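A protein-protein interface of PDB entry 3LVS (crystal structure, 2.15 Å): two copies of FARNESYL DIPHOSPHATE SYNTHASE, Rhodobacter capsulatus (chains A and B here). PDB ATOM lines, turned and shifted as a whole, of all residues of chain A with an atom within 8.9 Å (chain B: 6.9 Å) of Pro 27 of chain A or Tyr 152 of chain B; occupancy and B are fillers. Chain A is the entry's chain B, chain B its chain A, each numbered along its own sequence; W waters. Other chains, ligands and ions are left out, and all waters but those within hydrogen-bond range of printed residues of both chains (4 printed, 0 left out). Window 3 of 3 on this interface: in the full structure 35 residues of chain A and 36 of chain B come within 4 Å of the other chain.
The backbone carbonyl oxygen of Ser 145 of chain B lies close to the backbone NH of Val 151 of chain B (3.4 Å).
O of Gly 146 of chain B sits at hydrogen-bond distance from N of Val 151 of chain B, at 3.3 Å.
The backbone carbonyl oxygen (O) of Gly 146 of chain B is in hydrogen-bond range of the backbone NH (N) of Tyr 152 of chain B, 3.4 Å away.
O of Leu 26 of chain A lies within hydrogen-bond range of NH2 of Arg 32 of chain A (2.8 Å).
The backbone carbonyl oxygen (O) of Asp 113 of chain A is in hydrogen-bond range of the side-chain hydroxyl (OG1) of Thr 117 of chain A (2.8 Å).
The backbone carbonyl oxygen (O) of Ala 114 of chain A sits close to the side-chain hydroxyl (OG1) of Thr 117 of chain A (3.5 Å).
Among the printed residues, merely in contact across the chains: Leu 26 of chain A with Ala 147 of chain B (3.8 Å), Leu 26 of chain A with Glu 148 of chain B (3.8 Å), Pro 27 of chain A with Ala 147 of chain B (3.4 Å), Pro 27 of chain A with Glu 148 of chain B (3.7 Å), Pro 27 of chain A with Tyr 152 of chain B (3.6 Å), Leu 31 of chain A with Val 151 of chain B (3.9 Å), Leu 31 of chain A with Tyr 152 of chain B (3.9 Å), Met 35 of chain A with Ala 147 of chain B (3.6 Å), Leu 110 of chain A with Val 151 of chain B (3.5 Å), Leu 110 of chain A with Ala 155 of chain B (3.95 Å), Leu 110 of chain A with Ile 158 of chain B (3.9 Å), Ala 114 of chain A with Val 151 of chain B (3.7 Å), Thr 117 of chain A with Ser 145 of chain B (3.9 Å) and Thr 117 of chain A with Gly 146 of chain B (3.8 Å).
Pro 27 of chain A touches three residues of chain B.
Tyr 152 of chain B touches two residues of chain A.
No residue of chain A comes within 4 Å of Gly 149 of chain B.
Val 151 of chain B touches three residues of chain A.
No residue of chain A comes within 4 Å of Gly 153 of chain B.
Printed residues of chain A within 4 Å of Ala 155 of chain B: Leu 110.
Of the printed residues of chain B, Thr 117 of chain A touches Ser 145 and Gly 146.
Printed residues of chain B within 4 Å of Ala 114 of chain A: Val 151.
The nearest residue of chain A that does not touch Tyr 152 of chain B is Ala 28 of chain A (4.3 Å).
Printed residues of chain B that touch a printed residue of chain A: Ser 145, Gly 146, Ala 147, Glu 148, Val 151, Tyr 152, Ala 155 and Ile 158.
Of the 18 printed residues of chain A, 7 touch a printed residue of chain B.
Among the printed residues, 14 pairs touch across the chains.
No position is printed for both chains.
Of the 14 pairs that touch across the chains among the printed residues, none has its exchanged pair printed and touching as well.
Water W4 lies within hydrogen-bond range of OH of Tyr 152 of chain B (2.4 Å) and O of Ala 28 of chain A (2.6 Å).
Water W1 bridges the backbone carbonyl oxygen (O) of Ala 147 of chain B (2.7 Å) and the backbone carbonyl oxygen (O) of Pro 27 of chain A (2.8 Å).
Water W2 lies within hydrogen-bond range of the backbone NH (N) of Ala 147 of chain B and the backbone carbonyl oxygen (O) of Ala 114 of chain A.
Water W3 lies within hydrogen-bond range of the backbone carbonyl oxygen of Ser 145 of chain B and the side-chain hydroxyl of Thr 117 of chain A.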
ATOM      1  N   ALA A  22     -29.581  -8.613 -32.209  1.00  0.00           N
ATOM      2  CA  ALA A  22     -30.014  -7.264 -32.608  1.00  0.00           C
ATOM      3  C   ALA A  22     -29.440  -6.189 -31.690  1.00  0.00           C
ATOM      4  O   ALA A  22     -29.184  -5.072 -32.120  1.00  0.00           O
ATOM      5  CB  ALA A  22     -31.529  -7.173 -32.686  1.00  0.00           C
ATOM      6  N   ILE A  23     -29.223  -6.556 -30.431  1.00  0.00           N
ATOM      7  CA  ILE A  23     -28.638  -5.665 -29.438  1.00  0.00           C
ATOM      8  C   ILE A  23     -27.111  -5.613 -29.599  1.00  0.00           C
ATOM      9  O   ILE A  23     -26.500  -4.551 -29.450  1.00  0.00           O
ATOM     10  CB  ILE A  23     -29.076  -6.078 -28.002  1.00  0.00           C
ATOM     11  CG1 ILE A  23     -30.543  -5.668 -27.772  1.00  0.00           C
ATOM     12  CG2 ILE A  23     -28.139  -5.482 -26.919  1.00  0.00           C
ATOM     13  CD1 ILE A  23     -31.168  -6.177 -26.470  1.00  0.00           C
ATOM     14  N   GLY A  24     -26.518  -6.758 -29.944  1.00  0.00           N
ATOM     15  CA  GLY A  24     -25.081  -6.883 -30.205  1.00  0.00           C
ATOM     16  C   GLY A  24     -24.578  -6.045 -31.368  1.00  0.00           C
ATOM     17  O   GLY A  24     -23.398  -5.717 -31.428  1.00  0.00           O
ATOM     18  N   ARG A  25     -25.480  -5.689 -32.284  1.00  0.00           N
ATOM     19  CA  ARG A  25     -25.182  -4.757 -33.373  1.00  0.00           C
ATOM     20  C   ARG A  25     -24.902  -3.311 -32.923  1.00  0.00           C
ATOM     21  O   ARG A  25     -24.273  -2.547 -33.650  1.00  0.00           O
ATOM     22  CB  ARG A  25     -26.322  -4.762 -34.393  1.00  0.00           C
ATOM     23  CG  ARG A  25     -26.187  -5.799 -35.470  1.00  0.00           C
ATOM     24  CD  ARG A  25     -27.431  -5.829 -36.334  1.00  0.00           C
ATOM     25  NE  ARG A  25     -28.392  -6.796 -35.817  1.00  0.00           N
ATOM     26  CZ  ARG A  25     -29.384  -7.332 -36.525  1.00  0.00           C
ATOM     27  NH1 ARG A  25     -30.196  -8.211 -35.958  1.00  0.00           N
ATOM     28  NH2 ARG A  25     -29.568  -6.997 -37.798  1.00  0.00           N
ATOM     29  N   LEU A  26     -25.379  -2.938 -31.739  1.00  0.00           N
ATOM     30  CA  LEU A  26     -25.214  -1.574 -31.222  1.00  0.00           C
ATOM     31  C   LEU A  26     -23.791  -1.342 -30.698  1.00  0.00           C
ATOM     32  O   LEU A  26     -23.091  -2.316 -30.401  1.00  0.00           O
ATOM     33  CB  LEU A  26     -26.252  -1.312 -30.119  1.00  0.00           C
ATOM     34  CG  LEU A  26     -27.706  -1.446 -30.568  1.00  0.00           C
ATOM     35  CD1 LEU A  26     -28.587  -1.650 -29.355  1.00  0.00           C
ATOM     36  CD2 LEU A  26     -28.169  -0.237 -31.401  1.00  0.00           C
ATOM     37  N   PRO A  27     -23.352  -0.062 -30.598  1.00  0.00           N
ATOM     38  CA  PRO A  27     -22.049   0.245 -29.987  1.00  0.00           C
ATOM     39  C   PRO A  27     -21.916  -0.314 -28.570  1.00  0.00           C
ATOM     40  O   PRO A  27     -22.866  -0.234 -27.779  1.00  0.00           O
ATOM     41  CB  PRO A  27     -22.031   1.773 -29.940  1.00  0.00           C
ATOM     42  CG  PRO A  27     -22.919   2.214 -31.059  1.00  0.00           C
ATOM     43  CD  PRO A  27     -23.961   1.137 -31.225  1.00  0.00           C
ATOM     44  N   ALA A  28     -20.748  -0.882 -28.265  1.00  0.00           N
ATOM     45  CA  ALA A  28     -20.473  -1.472 -26.948  1.00  0.00           C
ATOM     46  C   ALA A  28     -20.521  -0.430 -25.819  1.00  0.00           C
ATOM     47  O   ALA A  28     -20.507   0.775 -26.078  1.00  0.00           O
ATOM     48  CB  ALA A  28     -19.128  -2.193 -26.964  1.00  0.00           C
ATOM     49  N   GLY A  29     -20.596  -0.894 -24.574  1.00  0.00           N
ATOM     50  CA  GLY A  29     -20.636   0.006 -23.423  1.00  0.00           C
ATOM     51  C   GLY A  29     -21.675  -0.375 -22.388  1.00  0.00           C
ATOM     52  O   GLY A  29     -22.403  -1.352 -22.566  1.00  0.00           O
ATOM     53  N   ASP A  30     -21.735   0.405 -21.306  1.00  0.00           N
ATOM     54  CA  ASP A  30     -22.662   0.164 -20.187  1.00  0.00           C
ATOM     55  C   ASP A  30     -24.141   0.181 -20.585  1.00  0.00           C
ATOM     56  O   ASP A  30     -24.913  -0.651 -20.109  1.00  0.00           O
ATOM     57  CB  ASP A  30     -22.424   1.177 -19.060  1.00  0.00           C
ATOM     58  CG  ASP A  30     -21.253   0.798 -18.166  1.00  0.00           C
ATOM     59  OD1 ASP A  30     -20.935  -0.407 -18.066  1.00  0.00           O
ATOM     60  OD2 ASP A  30     -20.652   1.707 -17.554  1.00  0.00           O
ATOM     61  N   LEU A  31     -24.509   1.135 -21.446  1.00  0.00           N
ATOM     62  CA  LEU A  31     -25.860   1.258 -21.992  1.00  0.00           C
ATOM     63  C   LEU A  31     -26.308  -0.050 -22.641  1.00  0.00           C
ATOM     64  O   LEU A  31     -27.338  -0.603 -22.253  1.00  0.00           O
ATOM     65  CB  LEU A  31     -25.936   2.411 -23.011  1.00  0.00           C
ATOM     66  CG  LEU A  31     -27.227   2.556 -23.833  1.00  0.00           C
ATOM     67  CD1 LEU A  31     -28.433   2.877 -22.950  1.00  0.00           C
ATOM     68  CD2 LEU A  31     -27.078   3.616 -24.933  1.00  0.00           C
ATOM     69  N   ARG A  32     -25.509  -0.548 -23.592  1.00  0.00           N
ATOM     70  CA  ARG A  32     -25.813  -1.780 -24.313  1.00  0.00           C
ATOM     71  C   ARG A  32     -25.882  -3.000 -23.398  1.00  0.00           C
ATOM     72  O   ARG A  32     -26.754  -3.848 -23.581  1.00  0.00           O
ATOM     73  CB  ARG A  32     -24.797  -2.024 -25.421  1.00  0.00           C
ATOM     74  CG  ARG A  32     -25.293  -2.979 -26.483  1.00  0.00           C
ATOM     75  CD  ARG A  32     -24.210  -3.321 -27.471  1.00  0.00           C
ATOM     76  NE  ARG A  32     -23.227  -4.253 -26.919  1.00  0.00           N
ATOM     77  CZ  ARG A  32     -22.172  -4.716 -27.588  1.00  0.00           C
ATOM     78  NH1 ARG A  32     -21.327  -5.557 -27.000  1.00  0.00           N
ATOM     79  NH2 ARG A  32     -21.959  -4.339 -28.847  1.00  0.00           N
ATOM     80  N   ASP A  33     -24.982  -3.082 -22.415  1.00  0.00           N
ATOM     81  CA  ASP A  33     -25.014  -4.185 -21.450  1.00  0.00           C
ATOM     82  C   ASP A  33     -26.338  -4.225 -20.682  1.00  0.00           C
ATOM     83  O   ASP A  33     -26.919  -5.292 -20.503  1.00  0.00           O
ATOM     84  CB  ASP A  33     -23.843  -4.094 -20.464  1.00  0.00           C
ATOM     85  CG  ASP A  33     -22.491  -4.135 -21.147  1.00  0.00           C
ATOM     86  OD1 ASP A  33     -21.524  -3.623 -20.546  1.00  0.00           O
ATOM     87  OD2 ASP A  33     -22.385  -4.662 -22.279  1.00  0.00           O
ATOM     88  N   MET A  35     -29.243  -2.744 -21.668  1.00  0.00           N
ATOM     89  CA  MET A  35     -30.259  -3.069 -22.671  1.00  0.00           C
ATOM     90  C   MET A  35     -30.334  -4.592 -22.852  1.00  0.00           C
ATOM     91  O   MET A  35     -31.415  -5.185 -22.748  1.00  0.00           O
ATOM     92  CB  MET A  35     -29.935  -2.389 -24.012  1.00  0.00           C
ATOM     93  CG  MET A  35     -30.042  -0.886 -24.004  1.00  0.00           C
ATOM     94  SD  MET A  35     -29.724  -0.135 -25.620  1.00  0.00           S
ATOM     95  CE  MET A  35     -30.998  -1.010 -26.524  1.00  0.00           C
ATOM     96  N   LEU A 110     -32.004   5.575 -19.305  1.00  0.00           N
ATOM     97  CA  LEU A 110     -31.431   5.537 -20.654  1.00  0.00           C
ATOM     98  C   LEU A 110     -31.600   4.203 -21.373  1.00  0.00           C
ATOM     99  O   LEU A 110     -31.933   4.184 -22.561  1.00  0.00           O
ATOM    100  CB  LEU A 110     -29.967   5.988 -20.664  1.00  0.00           C
ATOM    101  CG  LEU A 110     -29.730   7.486 -20.415  1.00  0.00           C
ATOM    102  CD1 LEU A 110     -28.251   7.789 -20.283  1.00  0.00           C
ATOM    103  CD2 LEU A 110     -30.370   8.374 -21.500  1.00  0.00           C
ATOM    104  N   ALA A 111     -31.365   3.099 -20.665  1.00  0.00           N
ATOM    105  CA  ALA A 111     -31.589   1.769 -21.221  1.00  0.00           C
ATOM    106  C   ALA A 111     -33.045   1.573 -21.668  1.00  0.00           C
ATOM    107  O   ALA A 111     -33.283   0.996 -22.728  1.00  0.00           O
ATOM    108  CB  ALA A 111     -31.178   0.683 -20.231  1.00  0.00           C
ATOM    109  N   ASP A 113     -35.217   4.079 -22.397  1.00  0.00           N
ATOM    110  CA  ASP A 113     -35.419   4.989 -23.527  1.00  0.00           C
ATOM    111  C   ASP A 113     -34.971   4.404 -24.862  1.00  0.00           C
ATOM    112  O   ASP A 113     -35.676   4.531 -25.864  1.00  0.00           O
ATOM    113  CB  ASP A 113     -34.679   6.298 -23.284  1.00  0.00           C
ATOM    114  CG  ASP A 113     -35.330   7.134 -22.217  1.00  0.00           C
ATOM    115  OD1 ASP A 113     -36.552   6.980 -22.036  1.00  0.00           O
ATOM    116  OD2 ASP A 113     -34.619   7.924 -21.552  1.00  0.00           O
ATOM    117  N   ALA A 114     -33.794   3.781 -24.853  1.00  0.00           N
ATOM    118  CA  ALA A 114     -33.173   3.203 -26.045  1.00  0.00           C
ATOM    119  C   ALA A 114     -33.894   1.938 -26.495  1.00  0.00           C
ATOM    120  O   ALA A 114     -34.125   1.768 -27.696  1.00  0.00           O
ATOM    121  CB  ALA A 114     -31.699   2.910 -25.791  1.00  0.00           C
ATOM    122  N   THR A 117     -36.828   2.934 -28.385  1.00  0.00           N
ATOM    123  CA  THR A 117     -36.391   3.286 -29.736  1.00  0.00           C
ATOM    124  C   THR A 117     -36.101   2.066 -30.585  1.00  0.00           C
ATOM    125  O   THR A 117     -36.499   2.026 -31.739  1.00  0.00           O
ATOM    126  CB  THR A 117     -35.154   4.191 -29.740  1.00  0.00           C
ATOM    127  OG1 THR A 117     -35.141   4.980 -28.548  1.00  0.00           O
ATOM    128  CG2 THR A 117     -35.205   5.127 -30.940  1.00  0.00           C
ATOM    129  N   SER B 145     -32.246   8.736 -32.668  1.00  0.00           N
ATOM    130  CA  SER B 145     -32.698   8.852 -31.278  1.00  0.00           C
ATOM    131  C   SER B 145     -32.163   7.811 -30.301  1.00  0.00           C
ATOM    132  O   SER B 145     -32.140   8.066 -29.107  1.00  0.00           O
ATOM    133  CB  SER B 145     -34.220   8.838 -31.229  1.00  0.00           C
ATOM    134  OG  SER B 145     -34.733   9.831 -32.119  1.00  0.00           O
ATOM    135  N   GLY B 146     -31.733   6.658 -30.794  1.00  0.00           N
ATOM    136  CA  GLY B 146     -31.543   5.509 -29.913  1.00  0.00           C
ATOM    137  C   GLY B 146     -30.134   5.255 -29.448  1.00  0.00           C
ATOM    138  O   GLY B 146     -29.370   6.194 -29.221  1.00  0.00           O
ATOM    139  N   ALA B 147     -29.799   3.967 -29.321  1.00  0.00           N
ATOM    140  CA  ALA B 147     -28.504   3.497 -28.806  1.00  0.00           C
ATOM    141  C   ALA B 147     -27.329   3.621 -29.804  1.00  0.00           C
ATOM    142  O   ALA B 147     -26.235   3.107 -29.554  1.00  0.00           O
ATOM    143  CB  ALA B 147     -28.630   2.053 -28.327  1.00  0.00           C
ATOM    144  N   GLU B 148     -27.567   4.277 -30.935  1.00  0.00           N
ATOM    145  CA  GLU B 148     -26.489   4.671 -31.840  1.00  0.00           C
ATOM    146  C   GLU B 148     -26.446   6.180 -31.965  1.00  0.00           C
ATOM    147  O   GLU B 148     -25.496   6.728 -32.519  1.00  0.00           O
ATOM    148  CB  GLU B 148     -26.688   4.091 -33.237  1.00  0.00           C
ATOM    149  CG  GLU B 148     -26.580   2.594 -33.321  1.00  0.00           C
ATOM    150  CD  GLU B 148     -26.971   2.057 -34.684  1.00  0.00           C
ATOM    151  OE1 GLU B 148     -26.529   0.932 -35.018  1.00  0.00           O
ATOM    152  OE2 GLU B 148     -27.715   2.757 -35.420  1.00  0.00           O
ATOM    153  N   GLY B 149     -27.483   6.848 -31.466  1.00  0.00           N
ATOM    154  CA  GLY B 149     -27.625   8.287 -31.634  1.00  0.00           C
ATOM    155  C   GLY B 149     -27.626   9.055 -30.330  1.00  0.00           C
ATOM    156  O   GLY B 149     -26.657   8.996 -29.552  1.00  0.00           O
ATOM    157  N   MET B 150     -28.737   9.754 -30.105  1.00  0.00           N
ATOM    158  CA  MET B 150     -28.937  10.672 -28.983  1.00  0.00           C
ATOM    159  C   MET B 150     -28.717  10.057 -27.613  1.00  0.00           C
ATOM    160  O   MET B 150     -27.983  10.617 -26.804  1.00  0.00           O
ATOM    161  CB  MET B 150     -30.338  11.261 -29.052  1.00  0.00           C
ATOM    162  CG  MET B 150     -30.575  12.435 -28.134  1.00  0.00           C
ATOM    163  SD  MET B 150     -32.306  12.934 -28.172  1.00  0.00           S
ATOM    164  CE  MET B 150     -33.029  11.490 -27.365  1.00  0.00           C
ATOM    165  N   VAL B 151     -29.354   8.912 -27.369  1.00  0.00           N
ATOM    166  CA  VAL B 151     -29.244   8.183 -26.095  1.00  0.00           C
ATOM    167  C   VAL B 151     -27.808   7.717 -25.822  1.00  0.00           C
ATOM    168  O   VAL B 151     -27.314   7.813 -24.693  1.00  0.00           O
ATOM    169  CB  VAL B 151     -30.246   6.983 -26.042  1.00  0.00           C
ATOM    170  CG1 VAL B 151     -30.015   6.116 -24.825  1.00  0.00           C
ATOM    171  CG2 VAL B 151     -31.679   7.491 -26.033  1.00  0.00           C
ATOM    172  N   TYR B 152     -27.152   7.220 -26.867  1.00  0.00           N
ATOM    173  CA  TYR B 152     -25.748   6.815 -26.816  1.00  0.00           C
ATOM    174  C   TYR B 152     -24.848   7.990 -26.418  1.00  0.00           C
ATOM    175  O   TYR B 152     -24.009   7.864 -25.508  1.00  0.00           O
ATOM    176  CB  TYR B 152     -25.328   6.265 -28.182  1.00  0.00           C
ATOM    177  CG  TYR B 152     -23.888   5.814 -28.296  1.00  0.00           C
ATOM    178  CD1 TYR B 152     -23.085   6.264 -29.345  1.00  0.00           C
ATOM    179  CD2 TYR B 152     -23.329   4.924 -27.364  1.00  0.00           C
ATOM    180  CE1 TYR B 152     -21.757   5.843 -29.470  1.00  0.00           C
ATOM    181  CE2 TYR B 152     -22.009   4.501 -27.474  1.00  0.00           C
ATOM    182  CZ  TYR B 152     -21.231   4.962 -28.530  1.00  0.00           C
ATOM    183  OH  TYR B 152     -19.931   4.541 -28.651  1.00  0.00           O
ATOM    184  N   GLY B 153     -25.051   9.117 -27.101  1.00  0.00           N
ATOM    185  CA  GLY B 153     -24.379  10.377 -26.804  1.00  0.00           C
ATOM    186  C   GLY B 153     -24.549  10.835 -25.363  1.00  0.00           C
ATOM    187  O   GLY B 153     -23.557  11.194 -24.716  1.00  0.00           O
ATOM    188  N   GLN B 154     -25.797  10.812 -24.873  1.00  0.00           N
ATOM    189  CA  GLN B 154     -26.093  11.143 -23.472  1.00  0.00           C
ATOM    190  C   GLN B 154     -25.391  10.200 -22.507  1.00  0.00           C
ATOM    191  O   GLN B 154     -24.857  10.639 -21.485  1.00  0.00           O
ATOM    192  CB  GLN B 154     -27.599  11.149 -23.193  1.00  0.00           C
ATOM    193  CG  GLN B 154     -28.189  12.542 -23.063  1.00  0.00           C
ATOM    194  CD  GLN B 154     -27.586  13.326 -21.908  1.00  0.00           C
ATOM    195  OE1 GLN B 154     -27.427  14.540 -21.989  1.00  0.00           O
ATOM    196  NE2 GLN B 154     -27.240  12.630 -20.831  1.00  0.00           N
ATOM    197  N   ALA B 155     -25.365   8.913 -22.841  1.00  0.00           N
ATOM    198  CA  ALA B 155     -24.691   7.924 -21.997  1.00  0.00           C
ATOM    199  C   ALA B 155     -23.180   8.164 -21.937  1.00  0.00           C
ATOM    200  O   ALA B 155     -22.558   7.978 -20.881  1.00  0.00           O
ATOM    201  CB  ALA B 155     -24.984   6.511 -22.486  1.00  0.00           C
ATOM    202  N   LEU B 156     -22.606   8.574 -23.072  1.00  0.00           N
ATOM    203  CA  LEU B 156     -21.182   8.895 -23.162  1.00  0.00           C
ATOM    204  C   LEU B 156     -20.877  10.143 -22.354  1.00  0.00           C
ATOM    205  O   LEU B 156     -19.877  10.190 -21.651  1.00  0.00           O
ATOM    206  CB  LEU B 156     -20.734   9.094 -24.616  1.00  0.00           C
ATOM    207  CG  LEU B 156     -20.582   7.871 -25.526  1.00  0.00           C
ATOM    208  CD1 LEU B 156     -20.272   8.315 -26.950  1.00  0.00           C
ATOM    209  CD2 LEU B 156     -19.532   6.890 -25.005  1.00  0.00           C
ATOM    210  N   ASP B 157     -21.770  11.126 -22.448  1.00  0.00           N
ATOM    211  CA  ASP B 157     -21.680  12.380 -21.709  1.00  0.00           C
ATOM    212  C   ASP B 157     -21.670  12.173 -20.190  1.00  0.00           C
ATOM    213  O   ASP B 157     -20.925  12.843 -19.475  1.00  0.00           O
ATOM    214  CB  ASP B 157     -22.841  13.289 -22.112  1.00  0.00           C
ATOM    215  CG  ASP B 157     -22.528  14.760 -21.946  1.00  0.00           C
ATOM    216  OD1 ASP B 157     -21.353  15.114 -21.727  1.00  0.00           O
ATOM    217  OD2 ASP B 157     -23.470  15.572 -22.050  1.00  0.00           O
ATOM    218  N   ILE B 158     -22.496  11.242 -19.717  1.00  0.00           N
ATOM    219  CA  ILE B 158     -22.557  10.876 -18.305  1.00  0.00           C
ATOM    220  C   ILE B 158     -21.285  10.131 -17.870  1.00  0.00           C
ATOM    221  O   ILE B 158     -20.717  10.424 -16.811  1.00  0.00           O
ATOM    222  CB  ILE B 158     -23.857  10.078 -17.999  1.00  0.00           C
ATOM    223  CG1 ILE B 158     -25.036  11.051 -17.890  1.00  0.00           C
ATOM    224  CG2 ILE B 158     -23.732   9.247 -16.717  1.00  0.00           C
ATOM    225  CD1 ILE B 158     -26.377  10.447 -18.216  1.00  0.00           C
ATOM    226  N   ARG B 174     -17.265  13.951 -31.196  1.00  0.00           N
ATOM    227  CA  ARG B 174     -17.933  12.680 -31.459  1.00  0.00           C
ATOM    228  C   ARG B 174     -19.084  12.453 -30.475  1.00  0.00           C
ATOM    229  O   ARG B 174     -20.085  11.815 -30.816  1.00  0.00           O
ATOM    230  CB  ARG B 174     -16.917  11.542 -31.387  1.00  0.00           C
ATOM    231  CG  ARG B 174     -17.070  10.483 -32.480  1.00  0.00           C
ATOM    232  CD  ARG B 174     -15.761  10.251 -33.263  1.00  0.00           C
ATOM    233  NE  ARG B 174     -14.555  10.617 -32.509  1.00  0.00           N
ATOM    234  CZ  ARG B 174     -13.810   9.776 -31.793  1.00  0.00           C
ATOM    235  NH1 ARG B 174     -14.128   8.490 -31.715  1.00  0.00           N
ATOM    236  NH2 ARG B 174     -12.741  10.227 -31.146  1.00  0.00           N
ATOM    237  N   LEU B 175     -18.930  12.998 -29.268  1.00  0.00           N
ATOM    238  CA  LEU B 175     -19.946  12.953 -28.216  1.00  0.00           C
ATOM    239  C   LEU B 175     -21.195  13.749 -28.601  1.00  0.00           C
ATOM    240  O   LEU B 175     -22.315  13.233 -28.541  1.00  0.00           O
ATOM    241  CB  LEU B 175     -19.352  13.488 -26.905  1.00  0.00           C
ATOM    242  CG  LEU B 175     -20.093  13.333 -25.573  1.00  0.00           C
ATOM    243  CD1 LEU B 175     -19.095  13.011 -24.470  1.00  0.00           C
ATOM    244  CD2 LEU B 175     -20.910  14.580 -25.231  1.00  0.00           C
ATOM    245  N   GLY B 178     -23.516  12.693 -31.451  1.00  0.00           N
ATOM    246  CA  GLY B 178     -24.570  11.864 -30.892  1.00  0.00           C
ATOM    247  C   GLY B 178     -25.602  12.682 -30.125  1.00  0.00           C
ATOM    248  O   GLY B 178     -26.786  12.697 -30.491  1.00  0.00           O
ATOM    249  N   LYS B 179     -25.140  13.385 -29.087  1.00  0.00           N
ATOM    250  CA  LYS B 179     -26.005  14.059 -28.112  1.00  0.00           C
ATOM    251  C   LYS B 179     -26.958  15.121 -28.670  1.00  0.00           C
ATOM    252  O   LYS B 179     -28.107  15.204 -28.227  1.00  0.00           O
ATOM    253  CB  LYS B 179     -25.171  14.666 -26.988  1.00  0.00           C
ATOM    254  CG  LYS B 179     -25.970  14.924 -25.743  1.00  0.00           C
ATOM    255  CD  LYS B 179     -25.383  16.043 -24.926  1.00  0.00           C
ATOM    256  CE  LYS B 179     -26.498  16.856 -24.300  1.00  0.00           C
ATOM    257  NZ  LYS B 179     -26.233  17.083 -22.863  1.00  0.00           N
HETATM  258  O   HOH W   1     -25.052   1.510 -27.720  1.00  0.00           O
HETATM  259  O   HOH W   2     -31.814   2.161 -29.755  1.00  0.00           O
HETATM  260  O   HOH W   3     -34.517   7.835 -27.760  1.00  0.00           O
HETATM  261  O   HOH W   4     -19.234   2.641 -27.314  1.00  0.00           O
